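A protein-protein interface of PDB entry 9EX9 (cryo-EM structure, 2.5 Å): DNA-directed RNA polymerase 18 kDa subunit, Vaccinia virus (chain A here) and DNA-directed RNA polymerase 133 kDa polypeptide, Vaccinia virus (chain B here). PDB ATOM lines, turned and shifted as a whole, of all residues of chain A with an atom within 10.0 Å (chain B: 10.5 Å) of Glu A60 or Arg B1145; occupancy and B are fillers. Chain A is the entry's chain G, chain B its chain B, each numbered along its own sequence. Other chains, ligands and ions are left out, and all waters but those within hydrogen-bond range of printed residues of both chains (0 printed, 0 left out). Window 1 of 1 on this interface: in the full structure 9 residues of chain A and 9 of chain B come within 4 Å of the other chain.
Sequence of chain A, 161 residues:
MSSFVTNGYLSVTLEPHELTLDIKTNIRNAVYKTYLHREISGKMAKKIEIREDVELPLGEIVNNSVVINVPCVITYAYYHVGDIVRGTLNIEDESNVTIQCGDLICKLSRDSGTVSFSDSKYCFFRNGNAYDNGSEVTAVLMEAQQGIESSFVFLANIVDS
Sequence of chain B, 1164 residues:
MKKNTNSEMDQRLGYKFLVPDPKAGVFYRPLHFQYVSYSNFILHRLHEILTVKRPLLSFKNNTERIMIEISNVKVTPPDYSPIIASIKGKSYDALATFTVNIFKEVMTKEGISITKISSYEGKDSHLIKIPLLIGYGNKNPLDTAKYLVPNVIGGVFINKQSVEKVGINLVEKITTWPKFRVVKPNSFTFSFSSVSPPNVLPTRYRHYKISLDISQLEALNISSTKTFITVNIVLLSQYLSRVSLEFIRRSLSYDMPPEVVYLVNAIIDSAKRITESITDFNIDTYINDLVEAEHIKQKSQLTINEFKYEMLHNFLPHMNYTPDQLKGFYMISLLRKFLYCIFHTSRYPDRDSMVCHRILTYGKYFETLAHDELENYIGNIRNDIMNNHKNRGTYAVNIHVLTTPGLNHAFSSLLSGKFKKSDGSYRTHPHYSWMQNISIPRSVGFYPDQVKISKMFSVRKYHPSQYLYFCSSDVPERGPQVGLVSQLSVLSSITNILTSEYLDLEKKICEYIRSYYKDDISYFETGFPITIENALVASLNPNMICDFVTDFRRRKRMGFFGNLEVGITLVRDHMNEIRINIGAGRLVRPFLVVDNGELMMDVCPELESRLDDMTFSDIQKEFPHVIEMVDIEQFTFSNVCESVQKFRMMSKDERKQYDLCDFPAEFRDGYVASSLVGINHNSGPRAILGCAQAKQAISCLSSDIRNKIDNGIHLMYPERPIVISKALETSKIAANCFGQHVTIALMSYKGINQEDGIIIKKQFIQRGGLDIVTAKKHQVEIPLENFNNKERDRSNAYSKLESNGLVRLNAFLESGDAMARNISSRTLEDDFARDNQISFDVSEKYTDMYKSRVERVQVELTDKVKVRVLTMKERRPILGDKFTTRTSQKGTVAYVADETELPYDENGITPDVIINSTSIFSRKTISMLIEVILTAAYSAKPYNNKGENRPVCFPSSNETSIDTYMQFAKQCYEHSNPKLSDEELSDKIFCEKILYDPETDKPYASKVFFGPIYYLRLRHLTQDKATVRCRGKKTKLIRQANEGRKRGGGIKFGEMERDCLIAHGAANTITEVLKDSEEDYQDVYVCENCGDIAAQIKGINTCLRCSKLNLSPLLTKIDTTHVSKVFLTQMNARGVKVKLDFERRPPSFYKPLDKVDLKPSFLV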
ATOM      1  N   TYR A   9     -23.876  -4.425  13.614  1.00  0.00           N
ATOM      2  CA  TYR A   9     -22.444  -4.632  13.740  1.00  0.00           C
ATOM      3  C   TYR A   9     -21.857  -3.602  14.691  1.00  0.00           C
ATOM      4  O   TYR A   9     -22.254  -2.434  14.681  1.00  0.00           O
ATOM      5  CB  TYR A   9     -21.753  -4.527  12.381  1.00  0.00           C
ATOM      6  CG  TYR A   9     -22.032  -5.677  11.452  1.00  0.00           C
ATOM      7  CD1 TYR A   9     -21.283  -6.839  11.514  1.00  0.00           C
ATOM      8  CD2 TYR A   9     -23.035  -5.597  10.501  1.00  0.00           C
ATOM      9  CE1 TYR A   9     -21.529  -7.891  10.662  1.00  0.00           C
ATOM     10  CE2 TYR A   9     -23.290  -6.644   9.644  1.00  0.00           C
ATOM     11  CZ  TYR A   9     -22.533  -7.789   9.728  1.00  0.00           C
ATOM     12  OH  TYR A   9     -22.780  -8.839   8.877  1.00  0.00           O
ATOM     13  N   SER A  11     -18.108  -2.044  15.677  1.00  0.00           N
ATOM     14  CA  SER A  11     -16.722  -1.959  15.246  1.00  0.00           C
ATOM     15  C   SER A  11     -15.807  -1.986  16.460  1.00  0.00           C
ATOM     16  O   SER A  11     -16.126  -1.415  17.504  1.00  0.00           O
ATOM     17  CB  SER A  11     -16.486  -0.686  14.435  1.00  0.00           C
ATOM     18  OG  SER A  11     -15.170  -0.655  13.915  1.00  0.00           O
ATOM     19  N   VAL A  12     -14.671  -2.667  16.323  1.00  0.00           N
ATOM     20  CA  VAL A  12     -13.719  -2.804  17.416  1.00  0.00           C
ATOM     21  C   VAL A  12     -12.315  -2.924  16.840  1.00  0.00           C
ATOM     22  O   VAL A  12     -12.125  -3.251  15.667  1.00  0.00           O
ATOM     23  CB  VAL A  12     -14.059  -4.018  18.305  1.00  0.00           C
ATOM     24  CG1 VAL A  12     -13.818  -5.313  17.549  1.00  0.00           C
ATOM     25  CG2 VAL A  12     -13.267  -3.978  19.592  1.00  0.00           C
ATOM     26  N   THR A  13     -11.321  -2.651  17.685  1.00  0.00           N
ATOM     27  CA  THR A  13      -9.919  -2.634  17.287  1.00  0.00           C
ATOM     28  C   THR A  13      -9.124  -3.616  18.137  1.00  0.00           C
ATOM     29  O   THR A  13      -9.258  -3.632  19.364  1.00  0.00           O
ATOM     30  CB  THR A  13      -9.326  -1.231  17.427  1.00  0.00           C
ATOM     31  OG1 THR A  13     -10.003  -0.334  16.541  1.00  0.00           O
ATOM     32  CG2 THR A  13      -7.846  -1.238  17.099  1.00  0.00           C
ATOM     33  N   LEU A  14      -8.290  -4.418  17.481  1.00  0.00           N
ATOM     34  CA  LEU A  14      -7.456  -5.416  18.130  1.00  0.00           C
ATOM     35  C   LEU A  14      -5.996  -5.207  17.753  1.00  0.00           C
ATOM     36  O   LEU A  14      -5.682  -4.692  16.674  1.00  0.00           O
ATOM     37  CB  LEU A  14      -7.867  -6.840  17.741  1.00  0.00           C
ATOM     38  CG  LEU A  14      -9.188  -7.383  18.285  1.00  0.00           C
ATOM     39  CD1 LEU A  14     -10.373  -6.725  17.610  1.00  0.00           C
ATOM     40  CD2 LEU A  14      -9.238  -8.884  18.105  1.00  0.00           C
ATOM     41  N   GLU A  15      -5.111  -5.614  18.655  1.00  0.00           N
ATOM     42  CA  GLU A  15      -3.675  -5.579  18.447  1.00  0.00           C
ATOM     43  C   GLU A  15      -3.184  -6.921  17.927  1.00  0.00           C
ATOM     44  O   GLU A  15      -3.824  -7.953  18.141  1.00  0.00           O
ATOM     45  CB  GLU A  15      -2.957  -5.242  19.754  1.00  0.00           C
ATOM     46  CG  GLU A  15      -3.421  -3.946  20.388  1.00  0.00           C
ATOM     47  CD  GLU A  15      -3.213  -2.747  19.487  1.00  0.00           C
ATOM     48  OE1 GLU A  15      -2.314  -2.800  18.623  1.00  0.00           O
ATOM     49  OE2 GLU A  15      -3.949  -1.751  19.639  1.00  0.00           O
ATOM     50  N   PRO A  16      -2.049  -6.950  17.227  1.00  0.00           N
ATOM     51  CA  PRO A  16      -1.573  -8.235  16.692  1.00  0.00           C
ATOM     52  C   PRO A  16      -1.359  -9.299  17.753  1.00  0.00           C
ATOM     53  O   PRO A  16      -1.641 -10.474  17.500  1.00  0.00           O
ATOM     54  CB  PRO A  16      -0.261  -7.852  15.995  1.00  0.00           C
ATOM     55  CG  PRO A  16      -0.421  -6.430  15.656  1.00  0.00           C
ATOM     56  CD  PRO A  16      -1.213  -5.829  16.774  1.00  0.00           C
ATOM     57  N   LEU A  19      -4.128 -11.820  18.341  1.00  0.00           N
ATOM     58  CA  LEU A  19      -4.557 -12.735  17.284  1.00  0.00           C
ATOM     59  C   LEU A  19      -4.007 -14.138  17.542  1.00  0.00           C
ATOM     60  O   LEU A  19      -3.241 -14.697  16.764  1.00  0.00           O
ATOM     61  CB  LEU A  19      -4.115 -12.216  15.921  1.00  0.00           C
ATOM     62  CG  LEU A  19      -4.670 -10.867  15.469  1.00  0.00           C
ATOM     63  CD1 LEU A  19      -4.134 -10.521  14.095  1.00  0.00           C
ATOM     64  CD2 LEU A  19      -6.184 -10.867  15.459  1.00  0.00           C
ATOM     65  N   LEU A  56     -18.049 -14.251  10.094  1.00  0.00           N
ATOM     66  CA  LEU A  56     -17.371 -13.028  10.505  1.00  0.00           C
ATOM     67  C   LEU A  56     -16.797 -12.320   9.280  1.00  0.00           C
ATOM     68  O   LEU A  56     -16.131 -12.961   8.461  1.00  0.00           O
ATOM     69  CB  LEU A  56     -16.257 -13.346  11.500  1.00  0.00           C
ATOM     70  CG  LEU A  56     -15.529 -12.150  12.110  1.00  0.00           C
ATOM     71  CD1 LEU A  56     -16.453 -11.370  13.025  1.00  0.00           C
ATOM     72  CD2 LEU A  56     -14.298 -12.604  12.864  1.00  0.00           C
ATOM     73  N   PRO A  57     -17.036 -11.021   9.108  1.00  0.00           N
ATOM     74  CA  PRO A  57     -16.439 -10.306   7.973  1.00  0.00           C
ATOM     75  C   PRO A  57     -14.927 -10.211   8.107  1.00  0.00           C
ATOM     76  O   PRO A  57     -14.346 -10.444   9.167  1.00  0.00           O
ATOM     77  CB  PRO A  57     -17.087  -8.920   8.035  1.00  0.00           C
ATOM     78  CG  PRO A  57     -18.280  -9.079   8.896  1.00  0.00           C
ATOM     79  CD  PRO A  57     -17.957 -10.158   9.865  1.00  0.00           C
ATOM     80  N   LEU A  58     -14.283  -9.857   6.997  1.00  0.00           N
ATOM     81  CA  LEU A  58     -12.839  -9.674   7.005  1.00  0.00           C
ATOM     82  C   LEU A  58     -12.455  -8.499   7.894  1.00  0.00           C
ATOM     83  O   LEU A  58     -13.225  -7.554   8.079  1.00  0.00           O
ATOM     84  CB  LEU A  58     -12.316  -9.432   5.589  1.00  0.00           C
ATOM     85  CG  LEU A  58     -12.363 -10.589   4.595  1.00  0.00           C
ATOM     86  CD1 LEU A  58     -11.923 -10.107   3.233  1.00  0.00           C
ATOM     87  CD2 LEU A  58     -11.489 -11.733   5.057  1.00  0.00           C
ATOM     88  N   GLY A  59     -11.247  -8.564   8.447  1.00  0.00           N
ATOM     89  CA  GLY A  59     -10.717  -7.472   9.243  1.00  0.00           C
ATOM     90  C   GLY A  59      -9.835  -6.554   8.410  1.00  0.00           C
ATOM     91  O   GLY A  59      -9.120  -6.999   7.519  1.00  0.00           O
ATOM     92  N   GLU A  60      -9.897  -5.263   8.720  1.00  0.00           N
ATOM     93  CA  GLU A  60      -9.146  -4.246   7.996  1.00  0.00           C
ATOM     94  C   GLU A  60      -7.865  -3.921   8.745  1.00  0.00           C
ATOM     95  O   GLU A  60      -7.901  -3.626   9.941  1.00  0.00           O
ATOM     96  CB  GLU A  60      -9.977  -2.978   7.824  1.00  0.00           C
ATOM     97  CG  GLU A  60     -11.281  -3.191   7.102  1.00  0.00           C
ATOM     98  CD  GLU A  60     -12.038  -1.899   6.897  1.00  0.00           C
ATOM     99  OE1 GLU A  60     -11.487  -0.829   7.230  1.00  0.00           O
ATOM    100  OE2 GLU A  60     -13.185  -1.954   6.404  1.00  0.00           O
ATOM    101  N   ILE A  61      -6.741  -3.961   8.044  1.00  0.00           N
ATOM    102  CA  ILE A  61      -5.449  -3.659   8.644  1.00  0.00           C
ATOM    103  C   ILE A  61      -5.205  -2.164   8.514  1.00  0.00           C
ATOM    104  O   ILE A  61      -5.184  -1.626   7.403  1.00  0.00           O
ATOM    105  CB  ILE A  61      -4.324  -4.465   7.980  1.00  0.00           C
ATOM    106  CG1 ILE A  61      -4.632  -5.959   8.067  1.00  0.00           C
ATOM    107  CG2 ILE A  61      -2.995  -4.156   8.646  1.00  0.00           C
ATOM    108  CD1 ILE A  61      -3.602  -6.835   7.421  1.00  0.00           C
ATOM    109  N   VAL A  62      -5.030  -1.491   9.647  1.00  0.00           N
ATOM    110  CA  VAL A  62      -4.779  -0.057   9.688  1.00  0.00           C
ATOM    111  C   VAL A  62      -3.517   0.168  10.504  1.00  0.00           C
ATOM    112  O   VAL A  62      -3.494  -0.120  11.705  1.00  0.00           O
ATOM    113  CB  VAL A  62      -5.960   0.714  10.295  1.00  0.00           C
ATOM    114  CG1 VAL A  62      -5.657   2.194  10.335  1.00  0.00           C
ATOM    115  CG2 VAL A  62      -7.223   0.449   9.502  1.00  0.00           C
ATOM    116  N   ASN A  63      -2.477   0.689   9.859  1.00  0.00           N
ATOM    117  CA  ASN A  63      -1.181   0.844  10.506  1.00  0.00           C
ATOM    118  C   ASN A  63      -0.744  -0.481  11.118  1.00  0.00           C
ATOM    119  O   ASN A  63      -0.404  -1.415  10.385  1.00  0.00           O
ATOM    120  CB  ASN A  63      -1.234   1.948  11.561  1.00  0.00           C
ATOM    121  CG  ASN A  63      -1.420   3.323  10.956  1.00  0.00           C
ATOM    122  OD1 ASN A  63      -0.902   3.613   9.881  1.00  0.00           O
ATOM    123  ND2 ASN A  63      -2.166   4.176  11.643  1.00  0.00           N
ATOM    124  N   ASN A  64      -0.754  -0.587  12.448  1.00  0.00           N
ATOM    125  CA  ASN A  64      -0.310  -1.788  13.144  1.00  0.00           C
ATOM    126  C   ASN A  64      -1.441  -2.474  13.900  1.00  0.00           C
ATOM    127  O   ASN A  64      -1.177  -3.235  14.836  1.00  0.00           O
ATOM    128  CB  ASN A  64       0.821  -1.451  14.112  1.00  0.00           C
ATOM    129  CG  ASN A  64       1.915  -0.644  13.468  1.00  0.00           C
ATOM    130  OD1 ASN A  64       2.174  -0.769  12.276  1.00  0.00           O
ATOM    131  ND2 ASN A  64       2.570   0.195  14.257  1.00  0.00           N
ATOM    132  N   SER A  65      -2.691  -2.227  13.521  1.00  0.00           N
ATOM    133  CA  SER A  65      -3.842  -2.731  14.250  1.00  0.00           C
ATOM    134  C   SER A  65      -4.850  -3.312  13.271  1.00  0.00           C
ATOM    135  O   SER A  65      -4.749  -3.126  12.057  1.00  0.00           O
ATOM    136  CB  SER A  65      -4.495  -1.624  15.084  1.00  0.00           C
ATOM    137  OG  SER A  65      -3.541  -0.971  15.902  1.00  0.00           O
ATOM    138  N   VAL A  66      -5.841  -4.016  13.813  1.00  0.00           N
ATOM    139  CA  VAL A  66      -6.876  -4.663  13.019  1.00  0.00           C
ATOM    140  C   VAL A  66      -8.230  -4.143  13.470  1.00  0.00           C
ATOM    141  O   VAL A  66      -8.454  -3.920  14.662  1.00  0.00           O
ATOM    142  CB  VAL A  66      -6.808  -6.197  13.148  1.00  0.00           C
ATOM    143  CG1 VAL A  66      -7.874  -6.852  12.292  1.00  0.00           C
ATOM    144  CG2 VAL A  66      -5.433  -6.691  12.759  1.00  0.00           C
ATOM    145  N   VAL A  67      -9.127  -3.938  12.511  1.00  0.00           N
ATOM    146  CA  VAL A  67     -10.472  -3.437  12.759  1.00  0.00           C
ATOM    147  C   VAL A  67     -11.460  -4.516  12.348  1.00  0.00           C
ATOM    148  O   VAL A  67     -11.388  -5.035  11.228  1.00  0.00           O
ATOM    149  CB  VAL A  67     -10.738  -2.131  11.990  1.00  0.00           C
ATOM    150  CG1 VAL A  67     -12.208  -1.770  12.043  1.00  0.00           C
ATOM    151  CG2 VAL A  67      -9.894  -1.012  12.559  1.00  0.00           C
ATOM    152  N   ILE A  68     -12.382  -4.848  13.247  1.00  0.00           N
ATOM    153  CA  ILE A  68     -13.318  -5.947  13.052  1.00  0.00           C
ATOM    154  C   ILE A  68     -14.732  -5.448  13.302  1.00  0.00           C
ATOM    155  O   ILE A  68     -14.975  -4.687  14.245  1.00  0.00           O
ATOM    156  CB  ILE A  68     -13.003  -7.132  13.984  1.00  0.00           C
ATOM    157  CG1 ILE A  68     -11.512  -7.456  13.954  1.00  0.00           C
ATOM    158  CG2 ILE A  68     -13.804  -8.349  13.572  1.00  0.00           C
ATOM    159  CD1 ILE A  68     -11.122  -8.587  14.871  1.00  0.00           C
ATOM    160  N   ASN A  69     -15.665  -5.885  12.461  1.00  0.00           N
ATOM    161  CA  ASN A  69     -17.091  -5.617  12.641  1.00  0.00           C
ATOM    162  C   ASN A  69     -17.734  -6.876  13.210  1.00  0.00           C
ATOM    163  O   ASN A  69     -18.003  -7.830  12.478  1.00  0.00           O
ATOM    164  CB  ASN A  69     -17.737  -5.218  11.321  1.00  0.00           C
ATOM    165  CG  ASN A  69     -17.125  -3.976  10.727  1.00  0.00           C
ATOM    166  OD1 ASN A  69     -16.097  -4.037  10.058  1.00  0.00           O
ATOM    167  ND2 ASN A  69     -17.759  -2.836  10.959  1.00  0.00           N
ATOM    168  N   ASP B1141     -14.453  14.008   7.876  1.00  0.00           N
ATOM    169  CA  ASP B1141     -15.325  12.849   7.964  1.00  0.00           C
ATOM    170  C   ASP B1141     -14.479  11.586   8.054  1.00  0.00           C
ATOM    171  O   ASP B1141     -13.263  11.611   7.864  1.00  0.00           O
ATOM    172  CB  ASP B1141     -16.260  12.775   6.758  1.00  0.00           C
ATOM    173  CG  ASP B1141     -17.121  14.012   6.611  1.00  0.00           C
ATOM    174  OD1 ASP B1141     -16.584  15.070   6.221  1.00  0.00           O
ATOM    175  OD2 ASP B1141     -18.337  13.924   6.879  1.00  0.00           O
ATOM    176  N   PHE B1142     -15.136  10.472   8.353  1.00  0.00           N
ATOM    177  CA  PHE B1142     -14.462   9.192   8.486  1.00  0.00           C
ATOM    178  C   PHE B1142     -15.225   8.135   7.706  1.00  0.00           C
ATOM    179  O   PHE B1142     -16.449   8.209   7.562  1.00  0.00           O
ATOM    180  CB  PHE B1142     -14.330   8.778   9.956  1.00  0.00           C
ATOM    181  CG  PHE B1142     -13.461   9.696  10.761  1.00  0.00           C
ATOM    182  CD1 PHE B1142     -13.998  10.795  11.400  1.00  0.00           C
ATOM    183  CD2 PHE B1142     -12.106   9.469  10.866  1.00  0.00           C
ATOM    184  CE1 PHE B1142     -13.200  11.640  12.131  1.00  0.00           C
ATOM    185  CE2 PHE B1142     -11.306  10.315  11.597  1.00  0.00           C
ATOM    186  CZ  PHE B1142     -11.854  11.399  12.228  1.00  0.00           C
ATOM    187  N   GLU B1143     -14.489   7.149   7.206  1.00  0.00           N
ATOM    188  CA  GLU B1143     -15.046   6.139   6.321  1.00  0.00           C
ATOM    189  C   GLU B1143     -15.730   5.049   7.133  1.00  0.00           C
ATOM    190  O   GLU B1143     -15.139   4.496   8.066  1.00  0.00           O
ATOM    191  CB  GLU B1143     -13.952   5.531   5.446  1.00  0.00           C
ATOM    192  CG  GLU B1143     -14.467   4.901   4.169  1.00  0.00           C
ATOM    193  CD  GLU B1143     -13.360   4.282   3.342  1.00  0.00           C
ATOM    194  OE1 GLU B1143     -12.369   3.807   3.934  1.00  0.00           O
ATOM    195  OE2 GLU B1143     -13.478   4.273   2.098  1.00  0.00           O
ATOM    196  N   ARG B1144     -16.964   4.728   6.754  1.00  0.00           N
ATOM    197  CA  ARG B1144     -17.750   3.698   7.421  1.00  0.00           C
ATOM    198  C   ARG B1144     -18.186   2.657   6.395  1.00  0.00           C
ATOM    199  O   ARG B1144     -19.373   2.341   6.279  1.00  0.00           O
ATOM    200  CB  ARG B1144     -18.959   4.316   8.133  1.00  0.00           C
ATOM    201  CG  ARG B1144     -18.762   4.554   9.628  1.00  0.00           C
ATOM    202  CD  ARG B1144     -17.490   5.327   9.921  1.00  0.00           C
ATOM    203  NE  ARG B1144     -17.342   5.645  11.337  1.00  0.00           N
ATOM    204  CZ  ARG B1144     -17.819   6.735  11.920  1.00  0.00           C
ATOM    205  NH1 ARG B1144     -18.519   7.633  11.247  1.00  0.00           N
ATOM    206  NH2 ARG B1144     -17.587   6.933  13.215  1.00  0.00           N
ATOM    207  N   ARG B1145     -17.229   2.142   5.631  1.00  0.00           N
ATOM    208  CA  ARG B1145     -17.548   1.194   4.577  1.00  0.00           C
ATOM    209  C   ARG B1145     -18.228  -0.040   5.168  1.00  0.00           C
ATOM    210  O   ARG B1145     -17.824  -0.521   6.232  1.00  0.00           O
ATOM    211  CB  ARG B1145     -16.281   0.782   3.826  1.00  0.00           C
ATOM    212  CG  ARG B1145     -15.221   0.142   4.708  1.00  0.00           C
ATOM    213  CD  ARG B1145     -13.914  -0.090   3.962  1.00  0.00           C
ATOM    214  NE  ARG B1145     -13.975  -1.226   3.049  1.00  0.00           N
ATOM    215  CZ  ARG B1145     -14.236  -1.147   1.751  1.00  0.00           C
ATOM    216  NH1 ARG B1145     -14.498   0.011   1.164  1.00  0.00           N
ATOM    217  NH2 ARG B1145     -14.232  -2.257   1.020  1.00  0.00           N
ATOM    218  N   PRO B1146     -19.250  -0.580   4.510  1.00  0.00           N
ATOM    219  CA  PRO B1146     -19.918  -1.776   5.029  1.00  0.00           C
ATOM    220  C   PRO B1146     -18.997  -2.980   4.984  1.00  0.00           C
ATOM    221  O   PRO B1146     -18.040  -3.012   4.197  1.00  0.00           O
ATOM    222  CB  PRO B1146     -21.117  -1.949   4.083  1.00  0.00           C
ATOM    223  CG  PRO B1146     -20.710  -1.270   2.832  1.00  0.00           C
ATOM    224  CD  PRO B1146     -19.855  -0.117   3.251  1.00  0.00           C
ATOM    225  N   PRO B1147     -19.256  -3.996   5.805  1.00  0.00           N
ATOM    226  CA  PRO B1147     -18.342  -5.141   5.872  1.00  0.00           C
ATOM    227  C   PRO B1147     -18.303  -5.922   4.567  1.00  0.00           C
ATOM    228  O   PRO B1147     -19.248  -5.908   3.778  1.00  0.00           O
ATOM    229  CB  PRO B1147     -18.922  -5.987   7.009  1.00  0.00           C
ATOM    230  CG  PRO B1147     -20.357  -5.617   7.057  1.00  0.00           C
ATOM    231  CD  PRO B1147     -20.423  -4.171   6.683  1.00  0.00           C
ATOM    232  N   SER B1148     -17.183  -6.608   4.350  1.00  0.00           N
ATOM    233  CA  SER B1148     -16.954  -7.398   3.150  1.00  0.00           C
ATOM    234  C   SER B1148     -16.564  -8.820   3.531  1.00  0.00           C
ATOM    235  O   SER B1148     -15.983  -9.059   4.593  1.00  0.00           O
ATOM    236  CB  SER B1148     -15.860  -6.774   2.282  1.00  0.00           C
ATOM    237  OG  SER B1148     -14.651  -6.652   3.005  1.00  0.00           O
ATOM    238  N   PHE B1149     -16.889  -9.764   2.649  1.00  0.00           N
ATOM    239  CA  PHE B1149     -16.689 -11.185   2.899  1.00  0.00           C
ATOM    240  C   PHE B1149     -15.914 -11.812   1.753  1.00  0.00           C
ATOM    241  O   PHE B1149     -16.106 -11.449   0.589  1.00  0.00           O
ATOM    242  CB  PHE B1149     -18.025 -11.904   3.064  1.00  0.00           C
ATOM    243  CG  PHE B1149     -18.876 -11.340   4.155  1.00  0.00           C
ATOM    244  CD1 PHE B1149     -19.712 -10.269   3.912  1.00  0.00           C
ATOM    245  CD2 PHE B1149     -18.836 -11.877   5.426  1.00  0.00           C
ATOM    246  CE1 PHE B1149     -20.493  -9.747   4.914  1.00  0.00           C
ATOM    247  CE2 PHE B1149     -19.613 -11.356   6.431  1.00  0.00           C
ATOM    248  CZ  PHE B1149     -20.443 -10.291   6.175  1.00  0.00           C
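The backbone carbonyl oxygen (O) of Glu A60 is in hydrogen-bond range of the backbone NH (N) of Val A67 (2.9 Å).
Of the 22 printed residues of chain A, 4 touch a printed residue of chain B. Among the printed residues, 6 pairs touch across the chains. Among the printed residues, Asp or Glu carboxylates within 4 Å of a Lys or Arg side-chain nitrogen of the other chain: Glu A60 with Arg B1145.
NE of Arg B1145 lies within salt-bridge range of OE2 of Glu A60 (3.5 Å). The backbone NH of Leu A58 sits at hydrogen-bond distance from the backbone carbonyl oxygen of Ser B1148.
Tyr A9 touches Phe B1149. CB of Pro A57 touches CB of Pro B1147, 3.6 Å away. CB of Pro A57 touches O of Ser B1148 (3.6 Å). Pro A57 touches Phe B1149 (CG to CE2, 3.6 Å).
Glu A60 touches just one residue of chain B: Arg B1145. Of the printed residues of chain A, Arg B1145 touches Glu A60. No residue of chain B comes within 4 Å of Gly A59. Ile A61 touches none of the printed residues of chain B. No residue of chain B comes within 4 Å of Val A62. No residue of chain B comes within 4 Å of Val A66. No residue of chain B comes within 4 Å of Val A67. No residue of chain A comes within 4 Å of Glu B1143. No residue of chain A comes within 4 Å of Pro B1146. Of the printed residues of chain B, Pro A57 touches Pro B1147 (3.6 Å), Ser B1148 (3.6 Å) and Phe B1149 (3.6 Å). Printed residues of chain B within 4 Å of Leu A58: Ser B1148 (3.1 Å). Of the printed residues of chain A, Pro B1147 touches Pro A57 (3.6 Å). Of the printed residues of chain A, Ser B1148 touches Pro A57 and Leu A58. Asn A63 touches none of the printed residues of chain B. Glu A15 touches none of the printed residues of chain B. The nearest residue of chain A that does not touch Arg B1145 is Asn A69 (5.3 Å). The nearest printed residue of chain A that does not touch Pro B1147 is Tyr A9 (4.04 Å).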
